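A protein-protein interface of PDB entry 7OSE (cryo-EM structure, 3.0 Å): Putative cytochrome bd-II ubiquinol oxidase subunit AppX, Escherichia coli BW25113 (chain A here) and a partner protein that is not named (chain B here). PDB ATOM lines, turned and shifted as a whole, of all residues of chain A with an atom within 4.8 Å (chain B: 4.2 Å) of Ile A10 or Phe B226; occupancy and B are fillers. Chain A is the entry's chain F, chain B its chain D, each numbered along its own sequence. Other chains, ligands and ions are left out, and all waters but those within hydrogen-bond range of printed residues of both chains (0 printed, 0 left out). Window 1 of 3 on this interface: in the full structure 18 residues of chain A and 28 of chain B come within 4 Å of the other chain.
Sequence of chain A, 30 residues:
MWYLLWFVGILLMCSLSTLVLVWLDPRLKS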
ATOM      1  N   TRP A   6      19.656 -20.618   3.874  1.00  0.00           N
ATOM      2  CA  TRP A   6      18.959 -20.799   5.142  1.00  0.00           C
ATOM      3  C   TRP A   6      19.653 -21.834   6.012  1.00  0.00           C
ATOM      4  O   TRP A   6      19.749 -21.663   7.230  1.00  0.00           O
ATOM      5  CB  TRP A   6      17.509 -21.213   4.904  1.00  0.00           C
ATOM      6  CG  TRP A   6      16.915 -21.878   6.107  1.00  0.00           C
ATOM      7  CD1 TRP A   6      16.338 -21.265   7.179  1.00  0.00           C
ATOM      8  CD2 TRP A   6      16.862 -23.285   6.374  1.00  0.00           C
ATOM      9  NE1 TRP A   6      15.921 -22.201   8.092  1.00  0.00           N
ATOM     10  CE2 TRP A   6      16.232 -23.449   7.621  1.00  0.00           C
ATOM     11  CE3 TRP A   6      17.284 -24.420   5.677  1.00  0.00           C
ATOM     12  CZ2 TRP A   6      16.012 -24.701   8.185  1.00  0.00           C
ATOM     13  CZ3 TRP A   6      17.065 -25.662   6.239  1.00  0.00           C
ATOM     14  CH2 TRP A   6      16.434 -25.793   7.480  1.00  0.00           C
ATOM     15  N   PHE A   7      20.114 -22.930   5.410  1.00  0.00           N
ATOM     16  CA  PHE A   7      20.800 -23.966   6.178  1.00  0.00           C
ATOM     17  C   PHE A   7      22.052 -23.409   6.845  1.00  0.00           C
ATOM     18  O   PHE A   7      22.255 -23.556   8.062  1.00  0.00           O
ATOM     19  CB  PHE A   7      21.143 -25.135   5.254  1.00  0.00           C
ATOM     20  CG  PHE A   7      21.730 -26.320   5.957  1.00  0.00           C
ATOM     21  CD1 PHE A   7      20.918 -27.215   6.630  1.00  0.00           C
ATOM     22  CD2 PHE A   7      23.092 -26.555   5.925  1.00  0.00           C
ATOM     23  CE1 PHE A   7      21.456 -28.312   7.271  1.00  0.00           C
ATOM     24  CE2 PHE A   7      23.635 -27.651   6.563  1.00  0.00           C
ATOM     25  CZ  PHE A   7      22.816 -28.530   7.237  1.00  0.00           C
ATOM     26  N   VAL A   8      22.895 -22.738   6.060  1.00  0.00           N
ATOM     27  CA  VAL A   8      24.114 -22.150   6.607  1.00  0.00           C
ATOM     28  C   VAL A   8      23.772 -21.090   7.646  1.00  0.00           C
ATOM     29  O   VAL A   8      24.430 -20.988   8.685  1.00  0.00           O
ATOM     30  CB  VAL A   8      24.986 -21.582   5.472  1.00  0.00           C
ATOM     31  CG1 VAL A   8      26.254 -20.976   6.031  1.00  0.00           C
ATOM     32  CG2 VAL A   8      25.326 -22.674   4.473  1.00  0.00           C
ATOM     33  N   GLY A   9      22.723 -20.302   7.396  1.00  0.00           N
ATOM     34  CA  GLY A   9      22.358 -19.249   8.326  1.00  0.00           C
ATOM     35  C   GLY A   9      21.854 -19.771   9.658  1.00  0.00           C
ATOM     36  O   GLY A   9      22.185 -19.223  10.710  1.00  0.00           O
ATOM     37  N   ILE A  10      21.036 -20.825   9.637  1.00  0.00           N
ATOM     38  CA  ILE A  10      20.531 -21.367  10.891  1.00  0.00           C
ATOM     39  C   ILE A  10      21.653 -22.040  11.669  1.00  0.00           C
ATOM     40  O   ILE A  10      21.729 -21.915  12.898  1.00  0.00           O
ATOM     41  CB  ILE A  10      19.340 -22.317  10.653  1.00  0.00           C
ATOM     42  CG1 ILE A  10      18.766 -22.789  11.989  1.00  0.00           C
ATOM     43  CG2 ILE A  10      19.738 -23.520   9.828  1.00  0.00           C
ATOM     44  CD1 ILE A  10      18.457 -21.670  12.956  1.00  0.00           C
ATOM     45  N   LEU A  11      22.559 -22.738  10.976  1.00  0.00           N
ATOM     46  CA  LEU A  11      23.711 -23.287  11.685  1.00  0.00           C
ATOM     47  C   LEU A  11      24.573 -22.174  12.275  1.00  0.00           C
ATOM     48  O   LEU A  11      25.087 -22.300  13.395  1.00  0.00           O
ATOM     49  CB  LEU A  11      24.532 -24.179  10.757  1.00  0.00           C
ATOM     50  CG  LEU A  11      23.952 -25.561  10.468  1.00  0.00           C
ATOM     51  CD1 LEU A  11      24.927 -26.382   9.645  1.00  0.00           C
ATOM     52  CD2 LEU A  11      23.614 -26.271  11.765  1.00  0.00           C
ATOM     53  N   LEU A  12      24.733 -21.073  11.539  1.00  0.00           N
ATOM     54  CA  LEU A  12      25.489 -19.933  12.045  1.00  0.00           C
ATOM     55  C   LEU A  12      24.832 -19.335  13.280  1.00  0.00           C
ATOM     56  O   LEU A  12      25.517 -19.006  14.253  1.00  0.00           O
ATOM     57  CB  LEU A  12      25.633 -18.880  10.946  1.00  0.00           C
ATOM     58  CG  LEU A  12      26.540 -17.665  11.161  1.00  0.00           C
ATOM     59  CD1 LEU A  12      27.148 -17.267   9.842  1.00  0.00           C
ATOM     60  CD2 LEU A  12      25.774 -16.483  11.736  1.00  0.00           C
ATOM     61  N   MET A  13      23.510 -19.166  13.252  1.00  0.00           N
ATOM     62  CA  MET A  13      22.806 -18.621  14.408  1.00  0.00           C
ATOM     63  C   MET A  13      22.953 -19.539  15.611  1.00  0.00           C
ATOM     64  O   MET A  13      23.171 -19.076  16.738  1.00  0.00           O
ATOM     65  CB  MET A  13      21.329 -18.412  14.077  1.00  0.00           C
ATOM     66  CG  MET A  13      21.067 -17.354  13.024  1.00  0.00           C
ATOM     67  SD  MET A  13      19.416 -17.489  12.311  1.00  0.00           S
ATOM     68  CE  MET A  13      18.402 -17.376  13.780  1.00  0.00           C
ATOM     69  N   CYS A  14      22.847 -20.850  15.385  1.00  0.00           N
ATOM     70  CA  CYS A  14      23.016 -21.810  16.467  1.00  0.00           C
ATOM     71  C   CYS A  14      24.405 -21.706  17.084  1.00  0.00           C
ATOM     72  O   CYS A  14      24.555 -21.636  18.312  1.00  0.00           O
ATOM     73  CB  CYS A  14      22.760 -23.221  15.937  1.00  0.00           C
ATOM     74  SG  CYS A  14      21.037 -23.535  15.498  1.00  0.00           S
ATOM     75  N   SER A  17      24.853 -18.396  19.048  1.00  0.00           N
ATOM     76  CA  SER A  17      24.205 -18.448  20.354  1.00  0.00           C
ATOM     77  C   SER A  17      25.002 -19.307  21.324  1.00  0.00           C
ATOM     78  O   SER A  17      25.189 -18.933  22.491  1.00  0.00           O
ATOM     79  CB  SER A  17      22.779 -18.975  20.212  1.00  0.00           C
ATOM     80  OG  SER A  17      22.018 -18.149  19.349  1.00  0.00           O
ATOM     81  N   PHE B  31      14.793 -25.643  18.029  1.00  0.00           N
ATOM     82  CA  PHE B  31      16.159 -25.180  17.823  1.00  0.00           C
ATOM     83  C   PHE B  31      16.753 -24.595  19.095  1.00  0.00           C
ATOM     84  O   PHE B  31      17.951 -24.760  19.343  1.00  0.00           O
ATOM     85  CB  PHE B  31      16.218 -24.170  16.681  1.00  0.00           C
ATOM     86  CG  PHE B  31      16.592 -24.782  15.365  1.00  0.00           C
ATOM     87  CD1 PHE B  31      17.897 -25.163  15.115  1.00  0.00           C
ATOM     88  CD2 PHE B  31      15.641 -24.995  14.386  1.00  0.00           C
ATOM     89  CE1 PHE B  31      18.249 -25.736  13.912  1.00  0.00           C
ATOM     90  CE2 PHE B  31      15.987 -25.567  13.180  1.00  0.00           C
ATOM     91  CZ  PHE B  31      17.293 -25.938  12.943  1.00  0.00           C
ATOM     92  N   LEU B  32      15.945 -23.930  19.921  1.00  0.00           N
ATOM     93  CA  LEU B  32      16.472 -23.454  21.197  1.00  0.00           C
ATOM     94  C   LEU B  32      16.826 -24.619  22.121  1.00  0.00           C
ATOM     95  O   LEU B  32      17.822 -24.561  22.855  1.00  0.00           O
ATOM     96  CB  LEU B  32      15.472 -22.503  21.849  1.00  0.00           C
ATOM     97  CG  LEU B  32      15.309 -21.224  21.026  1.00  0.00           C
ATOM     98  CD1 LEU B  32      14.269 -20.298  21.618  1.00  0.00           C
ATOM     99  CD2 LEU B  32      16.644 -20.512  20.892  1.00  0.00           C
ATOM    100  N   TYR B 192      11.290 -18.792  14.194  1.00  0.00           N
ATOM    101  CA  TYR B 192      12.413 -18.614  15.110  1.00  0.00           C
ATOM    102  C   TYR B 192      12.194 -17.411  16.017  1.00  0.00           C
ATOM    103  O   TYR B 192      12.454 -17.477  17.226  1.00  0.00           O
ATOM    104  CB  TYR B 192      13.711 -18.447  14.325  1.00  0.00           C
ATOM    105  CG  TYR B 192      14.132 -19.673  13.560  1.00  0.00           C
ATOM    106  CD1 TYR B 192      13.690 -20.934  13.933  1.00  0.00           C
ATOM    107  CD2 TYR B 192      14.975 -19.572  12.466  1.00  0.00           C
ATOM    108  CE1 TYR B 192      14.074 -22.056  13.236  1.00  0.00           C
ATOM    109  CE2 TYR B 192      15.365 -20.686  11.764  1.00  0.00           C
ATOM    110  CZ  TYR B 192      14.915 -21.927  12.154  1.00  0.00           C
ATOM    111  OH  TYR B 192      15.302 -23.041  11.450  1.00  0.00           O
ATOM    112  N   ILE B 222      19.983 -16.828  25.607  1.00  0.00           N
ATOM    113  CA  ILE B 222      19.798 -17.609  24.385  1.00  0.00           C
ATOM    114  C   ILE B 222      18.677 -17.014  23.547  1.00  0.00           C
ATOM    115  O   ILE B 222      18.819 -16.811  22.334  1.00  0.00           O
ATOM    116  CB  ILE B 222      19.511 -19.084  24.721  1.00  0.00           C
ATOM    117  CG1 ILE B 222      20.673 -19.706  25.488  1.00  0.00           C
ATOM    118  CG2 ILE B 222      19.248 -19.871  23.452  1.00  0.00           C
ATOM    119  CD1 ILE B 222      20.431 -21.138  25.907  1.00  0.00           C
ATOM    120  N   GLY B 223      17.545 -16.722  24.191  1.00  0.00           N
ATOM    121  CA  GLY B 223      16.420 -16.159  23.473  1.00  0.00           C
ATOM    122  C   GLY B 223      16.745 -14.821  22.846  1.00  0.00           C
ATOM    123  O   GLY B 223      16.355 -14.551  21.715  1.00  0.00           O
ATOM    124  N   SER B 224      17.486 -13.975  23.563  1.00  0.00           N
ATOM    125  CA  SER B 224      17.815 -12.655  23.043  1.00  0.00           C
ATOM    126  C   SER B 224      18.709 -12.749  21.814  1.00  0.00           C
ATOM    127  O   SER B 224      18.441 -12.108  20.790  1.00  0.00           O
ATOM    128  CB  SER B 224      18.483 -11.821  24.134  1.00  0.00           C
ATOM    129  OG  SER B 224      18.656 -10.486  23.705  1.00  0.00           O
ATOM    130  N   VAL B 225      19.775 -13.549  21.891  1.00  0.00           N
ATOM    131  CA  VAL B 225      20.687 -13.658  20.752  1.00  0.00           C
ATOM    132  C   VAL B 225      19.970 -14.269  19.552  1.00  0.00           C
ATOM    133  O   VAL B 225      20.035 -13.748  18.425  1.00  0.00           O
ATOM    134  CB  VAL B 225      21.933 -14.474  21.139  1.00  0.00           C
ATOM    135  CG1 VAL B 225      22.863 -14.615  19.948  1.00  0.00           C
ATOM    136  CG2 VAL B 225      22.654 -13.817  22.304  1.00  0.00           C
ATOM    137  N   PHE B 226      19.262 -15.380  19.782  1.00  0.00           N
ATOM    138  CA  PHE B 226      18.560 -16.047  18.695  1.00  0.00           C
ATOM    139  C   PHE B 226      17.494 -15.141  18.097  1.00  0.00           C
ATOM    140  O   PHE B 226      17.328 -15.094  16.875  1.00  0.00           O
ATOM    141  CB  PHE B 226      17.943 -17.348  19.204  1.00  0.00           C
ATOM    142  CG  PHE B 226      17.659 -18.351  18.128  1.00  0.00           C
ATOM    143  CD1 PHE B 226      18.682 -19.099  17.576  1.00  0.00           C
ATOM    144  CD2 PHE B 226      16.369 -18.554  17.676  1.00  0.00           C
ATOM    145  CE1 PHE B 226      18.425 -20.027  16.588  1.00  0.00           C
ATOM    146  CE2 PHE B 226      16.105 -19.481  16.689  1.00  0.00           C
ATOM    147  CZ  PHE B 226      17.135 -20.218  16.144  1.00  0.00           C
ATOM    148  N   GLY B 227      16.777 -14.399  18.941  1.00  0.00           N
ATOM    149  CA  GLY B 227      15.743 -13.513  18.447  1.00  0.00           C
ATOM    150  C   GLY B 227      16.293 -12.355  17.645  1.00  0.00           C
ATOM    151  O   GLY B 227      15.702 -11.961  16.643  1.00  0.00           O
ATOM    152  N   THR B 228      17.423 -11.788  18.069  1.00  0.00           N
ATOM    153  CA  THR B 228      18.020 -10.708  17.290  1.00  0.00           C
ATOM    154  C   THR B 228      18.435 -11.203  15.910  1.00  0.00           C
ATOM    155  O   THR B 228      18.100 -10.589  14.884  1.00  0.00           O
ATOM    156  CB  THR B 228      19.215 -10.115  18.033  1.00  0.00           C
ATOM    157  OG1 THR B 228      18.789  -9.627  19.310  1.00  0.00           O
ATOM    158  CG2 THR B 228      19.810  -8.969  17.236  1.00  0.00           C
ATOM    159  N   LEU B 229      19.148 -12.333  15.861  1.00  0.00           N
ATOM    160  CA  LEU B 229      19.562 -12.860  14.562  1.00  0.00           C
ATOM    161  C   LEU B 229      18.354 -13.203  13.695  1.00  0.00           C
ATOM    162  O   LEU B 229      18.308 -12.854  12.505  1.00  0.00           O
ATOM    163  CB  LEU B 229      20.459 -14.081  14.752  1.00  0.00           C
ATOM    164  CG  LEU B 229      21.791 -13.799  15.447  1.00  0.00           C
ATOM    165  CD1 LEU B 229      22.630 -15.061  15.545  1.00  0.00           C
ATOM    166  CD2 LEU B 229      22.548 -12.705  14.714  1.00  0.00           C
ATOM    167  N   ALA B 230      17.347 -13.850  14.286  1.00  0.00           N
ATOM    168  CA  ALA B 230      16.177 -14.261  13.525  1.00  0.00           C
ATOM    169  C   ALA B 230      15.344 -13.071  13.074  1.00  0.00           C
ATOM    170  O   ALA B 230      14.762 -13.114  11.990  1.00  0.00           O
ATOM    171  CB  ALA B 230      15.328 -15.221  14.354  1.00  0.00           C
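The backbone carbonyl oxygen (O) of Ile A10 sits at hydrogen-bond distance from the side-chain sulfur (SG) of Cys A14, 3.1 Å away.
The side-chain hydroxyl (OG) of Ser A17 lies within hydrogen-bond range of the backbone carbonyl oxygen (O) of Met A13 (3.0 Å).
Trp A6 touches Tyr B192 (NE1 to OH, 3.5 Å).
CG1 of Ile A10 touches CE1 of Phe B31 (3.6 Å).
Ile A10 touches Tyr B192 (CD1 to CE2, 3.5 Å).
CZ of Phe B226 touches CD1 of Ile A10, at 3.7 Å.
CE of Met A13 touches CE1 of Phe B226 (3.9 Å).
Leu B229 touches Met A13.
Met A13 touches Ala B230 (CE to N, 3.7 Å).
SG of Cys A14 touches CD1 of Phe B31, 3.6 Å away.
OG of Ser A17 touches CG1 of Val B225 (3.7 Å).
Ser A17 touches Phe B226.
Of the printed residues of chain B, Trp A6 touches Tyr B192 (3.5 Å).
Ile A10 touches just these residues of chain B: Phe B31 (3.6 Å), Tyr B192 (3.5 Å) and Phe B226 (3.7 Å).
Of the printed residues of chain B, Cys A14 touches Phe B31 (3.6 Å).
Printed residues of chain A within 4 Å of Phe B31: Ile A10 and Cys A14.
Printed residues of chain A within 4 Å of Tyr B192: Trp A6 (3.5 Å) and Ile A10 (3.5 Å).
Of chain A, only Ile A10, Met A13 and Ser A17 come within 4 Å of Phe B226.
Printed residues of chain A within 4 Å of Ala B230: Met A13.
The nearest printed residue of chain B that does not touch Ile A10 is Ala B230 (7.3 Å).
The nearest residue of chain A that does not touch Phe B226 is Cys A14 (4.5 Å).
Of the 12 printed residues of chain B, 6 touch a printed residue of chain A.
Among the printed residues, 10 pairs touch across the chains.
Among the printed residues, no Asp or Glu carboxylate lies within 4 Å of a Lys or Arg side-chain nitrogen of the other chain.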
